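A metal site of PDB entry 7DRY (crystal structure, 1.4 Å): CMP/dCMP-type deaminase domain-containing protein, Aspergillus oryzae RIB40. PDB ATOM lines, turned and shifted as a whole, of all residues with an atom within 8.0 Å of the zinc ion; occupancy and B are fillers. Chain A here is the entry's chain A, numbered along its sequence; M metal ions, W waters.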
ATOM      1  N   VAL A  28      17.452  -3.635  26.365  1.00  0.00           N
ATOM      2  CA  VAL A  28      16.830  -3.604  27.682  1.00  0.00           C
ATOM      3  C   VAL A  28      17.586  -4.579  28.574  1.00  0.00           C
ATOM      4  O   VAL A  28      18.174  -5.544  28.104  1.00  0.00           O
ATOM      5  CB  VAL A  28      15.330  -3.959  27.550  1.00  0.00           C
ATOM      6  CG1 VAL A  28      14.634  -4.086  28.901  1.00  0.00           C
ATOM      7  CG2 VAL A  28      14.609  -2.912  26.708  1.00  0.00           C
ATOM      8  N   THR A  53      18.490  -7.923  26.292  1.00  0.00           N
ATOM      9  CA  THR A  53      17.981  -8.171  24.943  1.00  0.00           C
ATOM     10  C   THR A  53      19.037  -8.845  24.092  1.00  0.00           C
ATOM     11  O   THR A  53      20.181  -8.392  24.012  1.00  0.00           O
ATOM     12  CB  THR A  53      17.629  -6.819  24.313  1.00  0.00           C
ATOM     13  OG1 THR A  53      16.612  -6.179  25.091  1.00  0.00           O
ATOM     14  CG2 THR A  53      17.148  -6.999  22.868  1.00  0.00           C
ATOM     15  N   THR A  60      15.299 -12.162  21.090  1.00  0.00           N
ATOM     16  CA  THR A  60      14.945 -12.392  22.483  1.00  0.00           C
ATOM     17  C   THR A  60      14.936 -11.085  23.268  1.00  0.00           C
ATOM     18  O   THR A  60      15.806 -10.220  23.071  1.00  0.00           O
ATOM     19  CB  THR A  60      15.917 -13.380  23.149  1.00  0.00           C
ATOM     20  OG1 THR A  60      17.265 -12.896  23.037  1.00  0.00           O
ATOM     21  CG2 THR A  60      15.806 -14.754  22.509  1.00  0.00           C
ATOM     22  N   HIS A  61      13.956 -10.941  24.156  1.00  0.00           N
ATOM     23  CA  HIS A  61      13.842  -9.778  25.014  1.00  0.00           C
ATOM     24  C   HIS A  61      14.576  -9.995  26.337  1.00  0.00           C
ATOM     25  O   HIS A  61      14.955 -11.117  26.685  1.00  0.00           O
ATOM     26  CB  HIS A  61      12.373  -9.470  25.274  1.00  0.00           C
ATOM     27  CG  HIS A  61      11.680  -8.830  24.112  1.00  0.00           C
ATOM     28  ND1 HIS A  61      10.439  -8.240  24.219  1.00  0.00           N
ATOM     29  CD2 HIS A  61      12.031  -8.720  22.811  1.00  0.00           C
ATOM     30  CE1 HIS A  61      10.074  -7.767  23.043  1.00  0.00           C
ATOM     31  NE2 HIS A  61      11.022  -8.057  22.158  1.00  0.00           N
ATOM     32  N   ALA A  62      14.750  -8.915  27.099  1.00  0.00           N
ATOM     33  CA  ALA A  62      15.527  -8.996  28.344  1.00  0.00           C
ATOM     34  C   ALA A  62      14.858  -9.909  29.360  1.00  0.00           C
ATOM     35  O   ALA A  62      15.523 -10.742  29.999  1.00  0.00           O
ATOM     36  CB  ALA A  62      15.682  -7.596  28.935  1.00  0.00           C
ATOM     37  N   GLU A  63      13.541  -9.720  29.582  1.00  0.00           N
ATOM     38  CA  GLU A  63      12.851 -10.532  30.587  1.00  0.00           C
ATOM     39  C   GLU A  63      12.827 -11.979  30.159  1.00  0.00           C
ATOM     40  O   GLU A  63      12.947 -12.886  30.999  1.00  0.00           O
ATOM     41  CB  GLU A  63      11.412 -10.012  30.760  1.00  0.00           C
ATOM     42  CG  GLU A  63      11.304  -8.512  31.056  1.00  0.00           C
ATOM     43  CD  GLU A  63      11.102  -7.657  29.809  1.00  0.00           C
ATOM     44  OE1 GLU A  63      11.988  -7.594  28.942  1.00  0.00           O
ATOM     45  OE2 GLU A  63      10.032  -7.044  29.682  1.00  0.00           O
ATOM     46  N   GLN A  64      12.649 -12.212  28.855  1.00  0.00           N
ATOM     47  CA  GLN A  64      12.728 -13.553  28.285  1.00  0.00           C
ATOM     48  C   GLN A  64      14.083 -14.189  28.582  1.00  0.00           C
ATOM     49  O   GLN A  64      14.156 -15.318  29.066  1.00  0.00           O
ATOM     50  CB  GLN A  64      12.516 -13.426  26.775  1.00  0.00           C
ATOM     51  CG  GLN A  64      12.617 -14.711  25.964  1.00  0.00           C
ATOM     52  CD  GLN A  64      12.343 -14.464  24.491  1.00  0.00           C
ATOM     53  OE1 GLN A  64      12.280 -13.320  24.033  1.00  0.00           O
ATOM     54  NE2 GLN A  64      12.159 -15.538  23.737  1.00  0.00           N
ATOM     55  N   VAL A  97      13.285  -3.974  35.297  1.00  0.00           N
ATOM     56  CA  VAL A  97      13.541  -3.981  33.857  1.00  0.00           C
ATOM     57  C   VAL A  97      13.503  -2.534  33.387  1.00  0.00           C
ATOM     58  O   VAL A  97      12.708  -1.743  33.902  1.00  0.00           O
ATOM     59  CB  VAL A  97      12.526  -4.894  33.138  1.00  0.00           C
ATOM     60  CG1 VAL A  97      11.104  -4.488  33.457  1.00  0.00           C
ATOM     61  CG2 VAL A  97      12.760  -4.946  31.656  1.00  0.00           C
ATOM     62  N   MET A  99      12.551  -1.008  30.638  1.00  0.00           N
ATOM     63  CA  MET A  99      11.320  -0.601  29.963  1.00  0.00           C
ATOM     64  C   MET A  99      10.150  -1.492  30.386  1.00  0.00           C
ATOM     65  O   MET A  99      10.345  -2.625  30.824  1.00  0.00           O
ATOM     66  CB  MET A  99      11.506  -0.647  28.443  1.00  0.00           C
ATOM     67  CG  MET A  99      12.638   0.246  27.938  1.00  0.00           C
ATOM     68  SD  MET A  99      12.715   0.370  26.149  1.00  0.00           S
ATOM     69  CE  MET A  99      11.307   1.429  25.794  1.00  0.00           C
ATOM     70  N   GLU A 100       8.944  -0.954  30.246  1.00  0.00           N
ATOM     71  CA  GLU A 100       7.729  -1.689  30.569  1.00  0.00           C
ATOM     72  C   GLU A 100       7.713  -3.032  29.840  1.00  0.00           C
ATOM     73  O   GLU A 100       7.990  -3.067  28.635  1.00  0.00           O
ATOM     74  CB  GLU A 100       6.527  -0.859  30.112  1.00  0.00           C
ATOM     75  CG  GLU A 100       5.181  -1.544  30.259  1.00  0.00           C
ATOM     76  CD  GLU A 100       4.070  -0.789  29.567  1.00  0.00           C
ATOM     77  OE1 GLU A 100       4.356   0.268  28.958  1.00  0.00           O
ATOM     78  OE2 GLU A 100       2.908  -1.243  29.602  1.00  0.00           O
ATOM     79  N   PRO A 101       7.391  -4.140  30.514  1.00  0.00           N
ATOM     80  CA  PRO A 101       7.300  -5.417  29.805  1.00  0.00           C
ATOM     81  C   PRO A 101       6.230  -5.406  28.731  1.00  0.00           C
ATOM     82  O   PRO A 101       5.122  -4.885  28.922  1.00  0.00           O
ATOM     83  CB  PRO A 101       6.961  -6.424  30.916  1.00  0.00           C
ATOM     84  CG  PRO A 101       6.540  -5.591  32.093  1.00  0.00           C
ATOM     85  CD  PRO A 101       7.233  -4.285  31.970  1.00  0.00           C
ATOM     86  N   CYS A 102       6.561  -5.982  27.582  1.00  0.00           N
ATOM     87  CA  CYS A 102       5.658  -5.930  26.447  1.00  0.00           C
ATOM     88  C   CYS A 102       4.472  -6.869  26.622  1.00  0.00           C
ATOM     89  O   CYS A 102       4.565  -7.948  27.238  1.00  0.00           O
ATOM     90  CB  CYS A 102       6.378  -6.238  25.127  1.00  0.00           C
ATOM     91  SG  CYS A 102       7.098  -7.925  24.975  1.00  0.00           S
ATOM     92  N   GLY A 103       3.329  -6.440  26.082  1.00  0.00           N
ATOM     93  CA  GLY A 103       2.147  -7.272  26.080  1.00  0.00           C
ATOM     94  C   GLY A 103       1.754  -7.721  24.684  1.00  0.00           C
ATOM     95  O   GLY A 103       0.813  -8.493  24.506  1.00  0.00           O
ATOM     96  N   LYS A 104       2.498  -7.226  23.699  1.00  0.00           N
ATOM     97  CA  LYS A 104       2.306  -7.540  22.291  1.00  0.00           C
ATOM     98  C   LYS A 104       3.671  -7.435  21.623  1.00  0.00           C
ATOM     99  O   LYS A 104       4.472  -6.581  21.998  1.00  0.00           O
ATOM    100  CB  LYS A 104       1.323  -6.555  21.638  1.00  0.00           C
ATOM    101  CG  LYS A 104       0.981  -6.885  20.196  1.00  0.00           C
ATOM    102  CD  LYS A 104      -0.413  -6.385  19.838  1.00  0.00           C
ATOM    103  CE  LYS A 104      -0.586  -6.275  18.326  1.00  0.00           C
ATOM    104  NZ  LYS A 104      -0.368  -4.886  17.839  1.00  0.00           N
ATOM    105  N   ARG A 105       3.941  -8.310  20.668  1.00  0.00           N
ATOM    106  CA  ARG A 105       5.191  -8.288  19.934  1.00  0.00           C
ATOM    107  C   ARG A 105       4.914  -8.330  18.441  1.00  0.00           C
ATOM    108  O   ARG A 105       3.910  -8.878  17.998  1.00  0.00           O
ATOM    109  CB  ARG A 105       6.117  -9.458  20.336  1.00  0.00           C
ATOM    110  CG  ARG A 105       6.689  -9.293  21.731  1.00  0.00           C
ATOM    111  CD  ARG A 105       7.681 -10.403  22.087  1.00  0.00           C
ATOM    112  NE  ARG A 105       8.812 -10.427  21.173  1.00  0.00           N
ATOM    113  CZ  ARG A 105       9.923 -11.133  21.365  1.00  0.00           C
ATOM    114  NH1 ARG A 105      10.899 -11.089  20.461  1.00  0.00           N
ATOM    115  NH2 ARG A 105      10.058 -11.893  22.443  1.00  0.00           N
ATOM    116  N   ASN A 109       6.514 -14.204  18.748  1.00  0.00           N
ATOM    117  CA  ASN A 109       6.984 -14.702  20.040  1.00  0.00           C
ATOM    118  C   ASN A 109       6.074 -14.231  21.166  1.00  0.00           C
ATOM    119  O   ASN A 109       5.501 -13.142  21.128  1.00  0.00           O
ATOM    120  CB  ASN A 109       8.421 -14.227  20.289  1.00  0.00           C
ATOM    121  CG  ASN A 109       9.398 -14.813  19.296  1.00  0.00           C
ATOM    122  OD1 ASN A 109       9.702 -16.005  19.328  1.00  0.00           O
ATOM    123  ND2 ASN A 109       9.896 -13.979  18.396  1.00  0.00           N
ATOM    124  N   LEU A 110       5.952 -15.086  22.176  1.00  0.00           N
ATOM    125  CA  LEU A 110       5.098 -14.776  23.313  1.00  0.00           C
ATOM    126  C   LEU A 110       5.591 -13.504  23.984  1.00  0.00           C
ATOM    127  O   LEU A 110       6.798 -13.374  24.237  1.00  0.00           O
ATOM    128  CB  LEU A 110       5.143 -15.915  24.321  1.00  0.00           C
ATOM    129  CG  LEU A 110       4.153 -15.786  25.484  1.00  0.00           C
ATOM    130  CD1 LEU A 110       2.715 -15.902  24.972  1.00  0.00           C
ATOM    131  CD2 LEU A 110       4.415 -16.841  26.555  1.00  0.00           C
ATOM    132  N   PRO A 111       4.728 -12.526  24.267  1.00  0.00           N
ATOM    133  CA  PRO A 111       5.190 -11.299  24.894  1.00  0.00           C
ATOM    134  C   PRO A 111       5.658 -11.527  26.331  1.00  0.00           C
ATOM    135  O   PRO A 111       5.403 -12.568  26.954  1.00  0.00           O
ATOM    136  CB  PRO A 111       3.984 -10.353  24.820  1.00  0.00           C
ATOM    137  CG  PRO A 111       3.151 -10.912  23.701  1.00  0.00           C
ATOM    138  CD  PRO A 111       3.327 -12.409  23.805  1.00  0.00           C
ATOM    139  N   CYS A 112       6.344 -10.531  26.857  1.00  0.00           N
ATOM    140  CA  CYS A 112       7.063 -10.700  28.119  1.00  0.00           C
ATOM    141  C   CYS A 112       6.088 -10.760  29.297  1.00  0.00           C
ATOM    142  O   CYS A 112       6.319 -11.495  30.255  1.00  0.00           O
ATOM    143  CB  CYS A 112       8.036  -9.545  28.284  1.00  0.00           C
ATOM    144  SG  CYS A 112       9.526  -9.755  27.288  1.00  0.00           S
ATOM    145  N   VAL A 113       4.998  -9.995  29.232  1.00  0.00           N
ATOM    146  CA  VAL A 113       4.027 -10.019  30.332  1.00  0.00           C
ATOM    147  C   VAL A 113       3.446 -11.418  30.495  1.00  0.00           C
ATOM    148  O   VAL A 113       3.251 -11.901  31.616  1.00  0.00           O
ATOM    149  CB  VAL A 113       2.946  -8.947  30.138  1.00  0.00           C
ATOM    150  CG1 VAL A 113       1.772  -9.192  31.079  1.00  0.00           C
ATOM    151  CG2 VAL A 113       3.522  -7.570  30.378  1.00  0.00           C
ATOM    152  N   GLN A 114       3.195 -12.106  29.372  1.00  0.00           N
ATOM    153  CA  GLN A 114       2.680 -13.466  29.455  1.00  0.00           C
ATOM    154  C   GLN A 114       3.708 -14.427  30.036  1.00  0.00           C
ATOM    155  O   GLN A 114       3.349 -15.335  30.791  1.00  0.00           O
ATOM    156  CB  GLN A 114       2.206 -13.912  28.070  1.00  0.00           C
ATOM    157  CG  GLN A 114       0.901 -13.232  27.596  1.00  0.00           C
ATOM    158  CD  GLN A 114       1.123 -11.897  26.875  1.00  0.00           C
ATOM    159  OE1 GLN A 114       2.086 -11.184  27.156  1.00  0.00           O
ATOM    160  NE2 GLN A 114       0.236 -11.565  25.949  1.00  0.00           N
ATOM    161  N   ARG A 115       4.988 -14.247  29.683  1.00  0.00           N
ATOM    162  CA  ARG A 115       6.059 -15.034  30.314  1.00  0.00           C
ATOM    163  C   ARG A 115       6.100 -14.801  31.816  1.00  0.00           C
ATOM    164  O   ARG A 115       6.352 -15.723  32.593  1.00  0.00           O
ATOM    165  CB  ARG A 115       7.419 -14.709  29.704  1.00  0.00           C
ATOM    166  CG  ARG A 115       7.559 -15.040  28.244  1.00  0.00           C
ATOM    167  CD  ARG A 115       8.979 -14.691  27.747  1.00  0.00           C
ATOM    168  NE  ARG A 115       8.961 -14.617  26.299  1.00  0.00           N
ATOM    169  CZ  ARG A 115       9.081 -15.670  25.494  1.00  0.00           C
ATOM    170  NH1 ARG A 115       8.995 -15.511  24.183  1.00  0.00           N
ATOM    171  NH2 ARG A 115       9.298 -16.874  25.995  1.00  0.00           N
ATOM    172  N   ILE A 116       5.867 -13.554  32.235  1.00  0.00           N
ATOM    173  CA  ILE A 116       5.869 -13.224  33.659  1.00  0.00           C
ATOM    174  C   ILE A 116       4.652 -13.834  34.360  1.00  0.00           C
ATOM    175  O   ILE A 116       4.760 -14.435  35.429  1.00  0.00           O
ATOM    176  CB  ILE A 116       5.928 -11.690  33.841  1.00  0.00           C
ATOM    177  CG1 ILE A 116       7.299 -11.162  33.426  1.00  0.00           C
ATOM    178  CG2 ILE A 116       5.573 -11.293  35.278  1.00  0.00           C
ATOM    179  CD1 ILE A 116       7.279  -9.666  33.147  1.00  0.00           C
ATOM    180  N   PRO A 137       6.946   0.027  26.143  1.00  0.00           N
ATOM    181  CA  PRO A 137       7.545  -1.293  26.002  1.00  0.00           C
ATOM    182  C   PRO A 137       8.761  -1.265  25.092  1.00  0.00           C
ATOM    183  O   PRO A 137       8.962  -0.337  24.305  1.00  0.00           O
ATOM    184  CB  PRO A 137       6.425  -2.117  25.361  1.00  0.00           C
ATOM    185  CG  PRO A 137       5.659  -1.105  24.551  1.00  0.00           C
ATOM    186  CD  PRO A 137       5.697   0.164  25.357  1.00  0.00           C
ATOM    187  N   GLY A 138       9.566  -2.320  25.188  1.00  0.00           N
ATOM    188  CA  GLY A 138      10.713  -2.491  24.324  1.00  0.00           C
ATOM    189  C   GLY A 138      10.327  -3.072  22.981  1.00  0.00           C
ATOM    190  O   GLY A 138      10.860  -4.098  22.557  1.00  0.00           O
ATOM    191  N   THR A 139       9.379  -2.402  22.311  1.00  0.00           N
ATOM    192  CA  THR A 139       8.877  -2.792  20.998  1.00  0.00           C
ATOM    193  C   THR A 139       8.440  -1.532  20.295  1.00  0.00           C
ATOM    194  O   THR A 139       8.256  -0.475  20.915  1.00  0.00           O
ATOM    195  CB  THR A 139       7.619  -3.667  21.091  1.00  0.00           C
ATOM    196  OG1 THR A 139       6.558  -2.898  21.681  1.00  0.00           O
ATOM    197  CG2 THR A 139       7.852  -4.936  21.883  1.00  0.00           C
HETATM  198 ZN    ZN M   1       9.162  -8.028  25.799  1.00  0.00          ZN
HETATM  199  O   HOH W   1       9.771  -5.640  26.336  1.00  0.00           O
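A ring nitrogen (ND1) of His 61 is bound to the zinc ion (2.0 Å).
The zinc ion is bound by the side-chain sulfur (SG) of Cys 102 (2.2 Å).
The zinc ion is bound by SG of Cys 112 (2.3 Å).
The zinc ion is bound by water W1 (2.5 Å).
The zinc ion has four donor atoms within binding distance.
A ring nitrogen (NE2) of His 61 sits close to the guanidinium group (NE) of Arg 105 (3.4 Å).
OE1 of Gln 64 is in hydrogen-bond range of N of His 61.
N of Val 113 lies within hydrogen-bond range of O of Cys 102, 2.9 Å away.
SG of Cys 112 sits close to OE2 of Glu 63 (3.7 Å).
Within 4 Å of the zinc ion: His 61, Cys 102 and Cys 112.
The nearest printed residue that does not touch the zinc ion is Glu 63 (4.1 Å).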
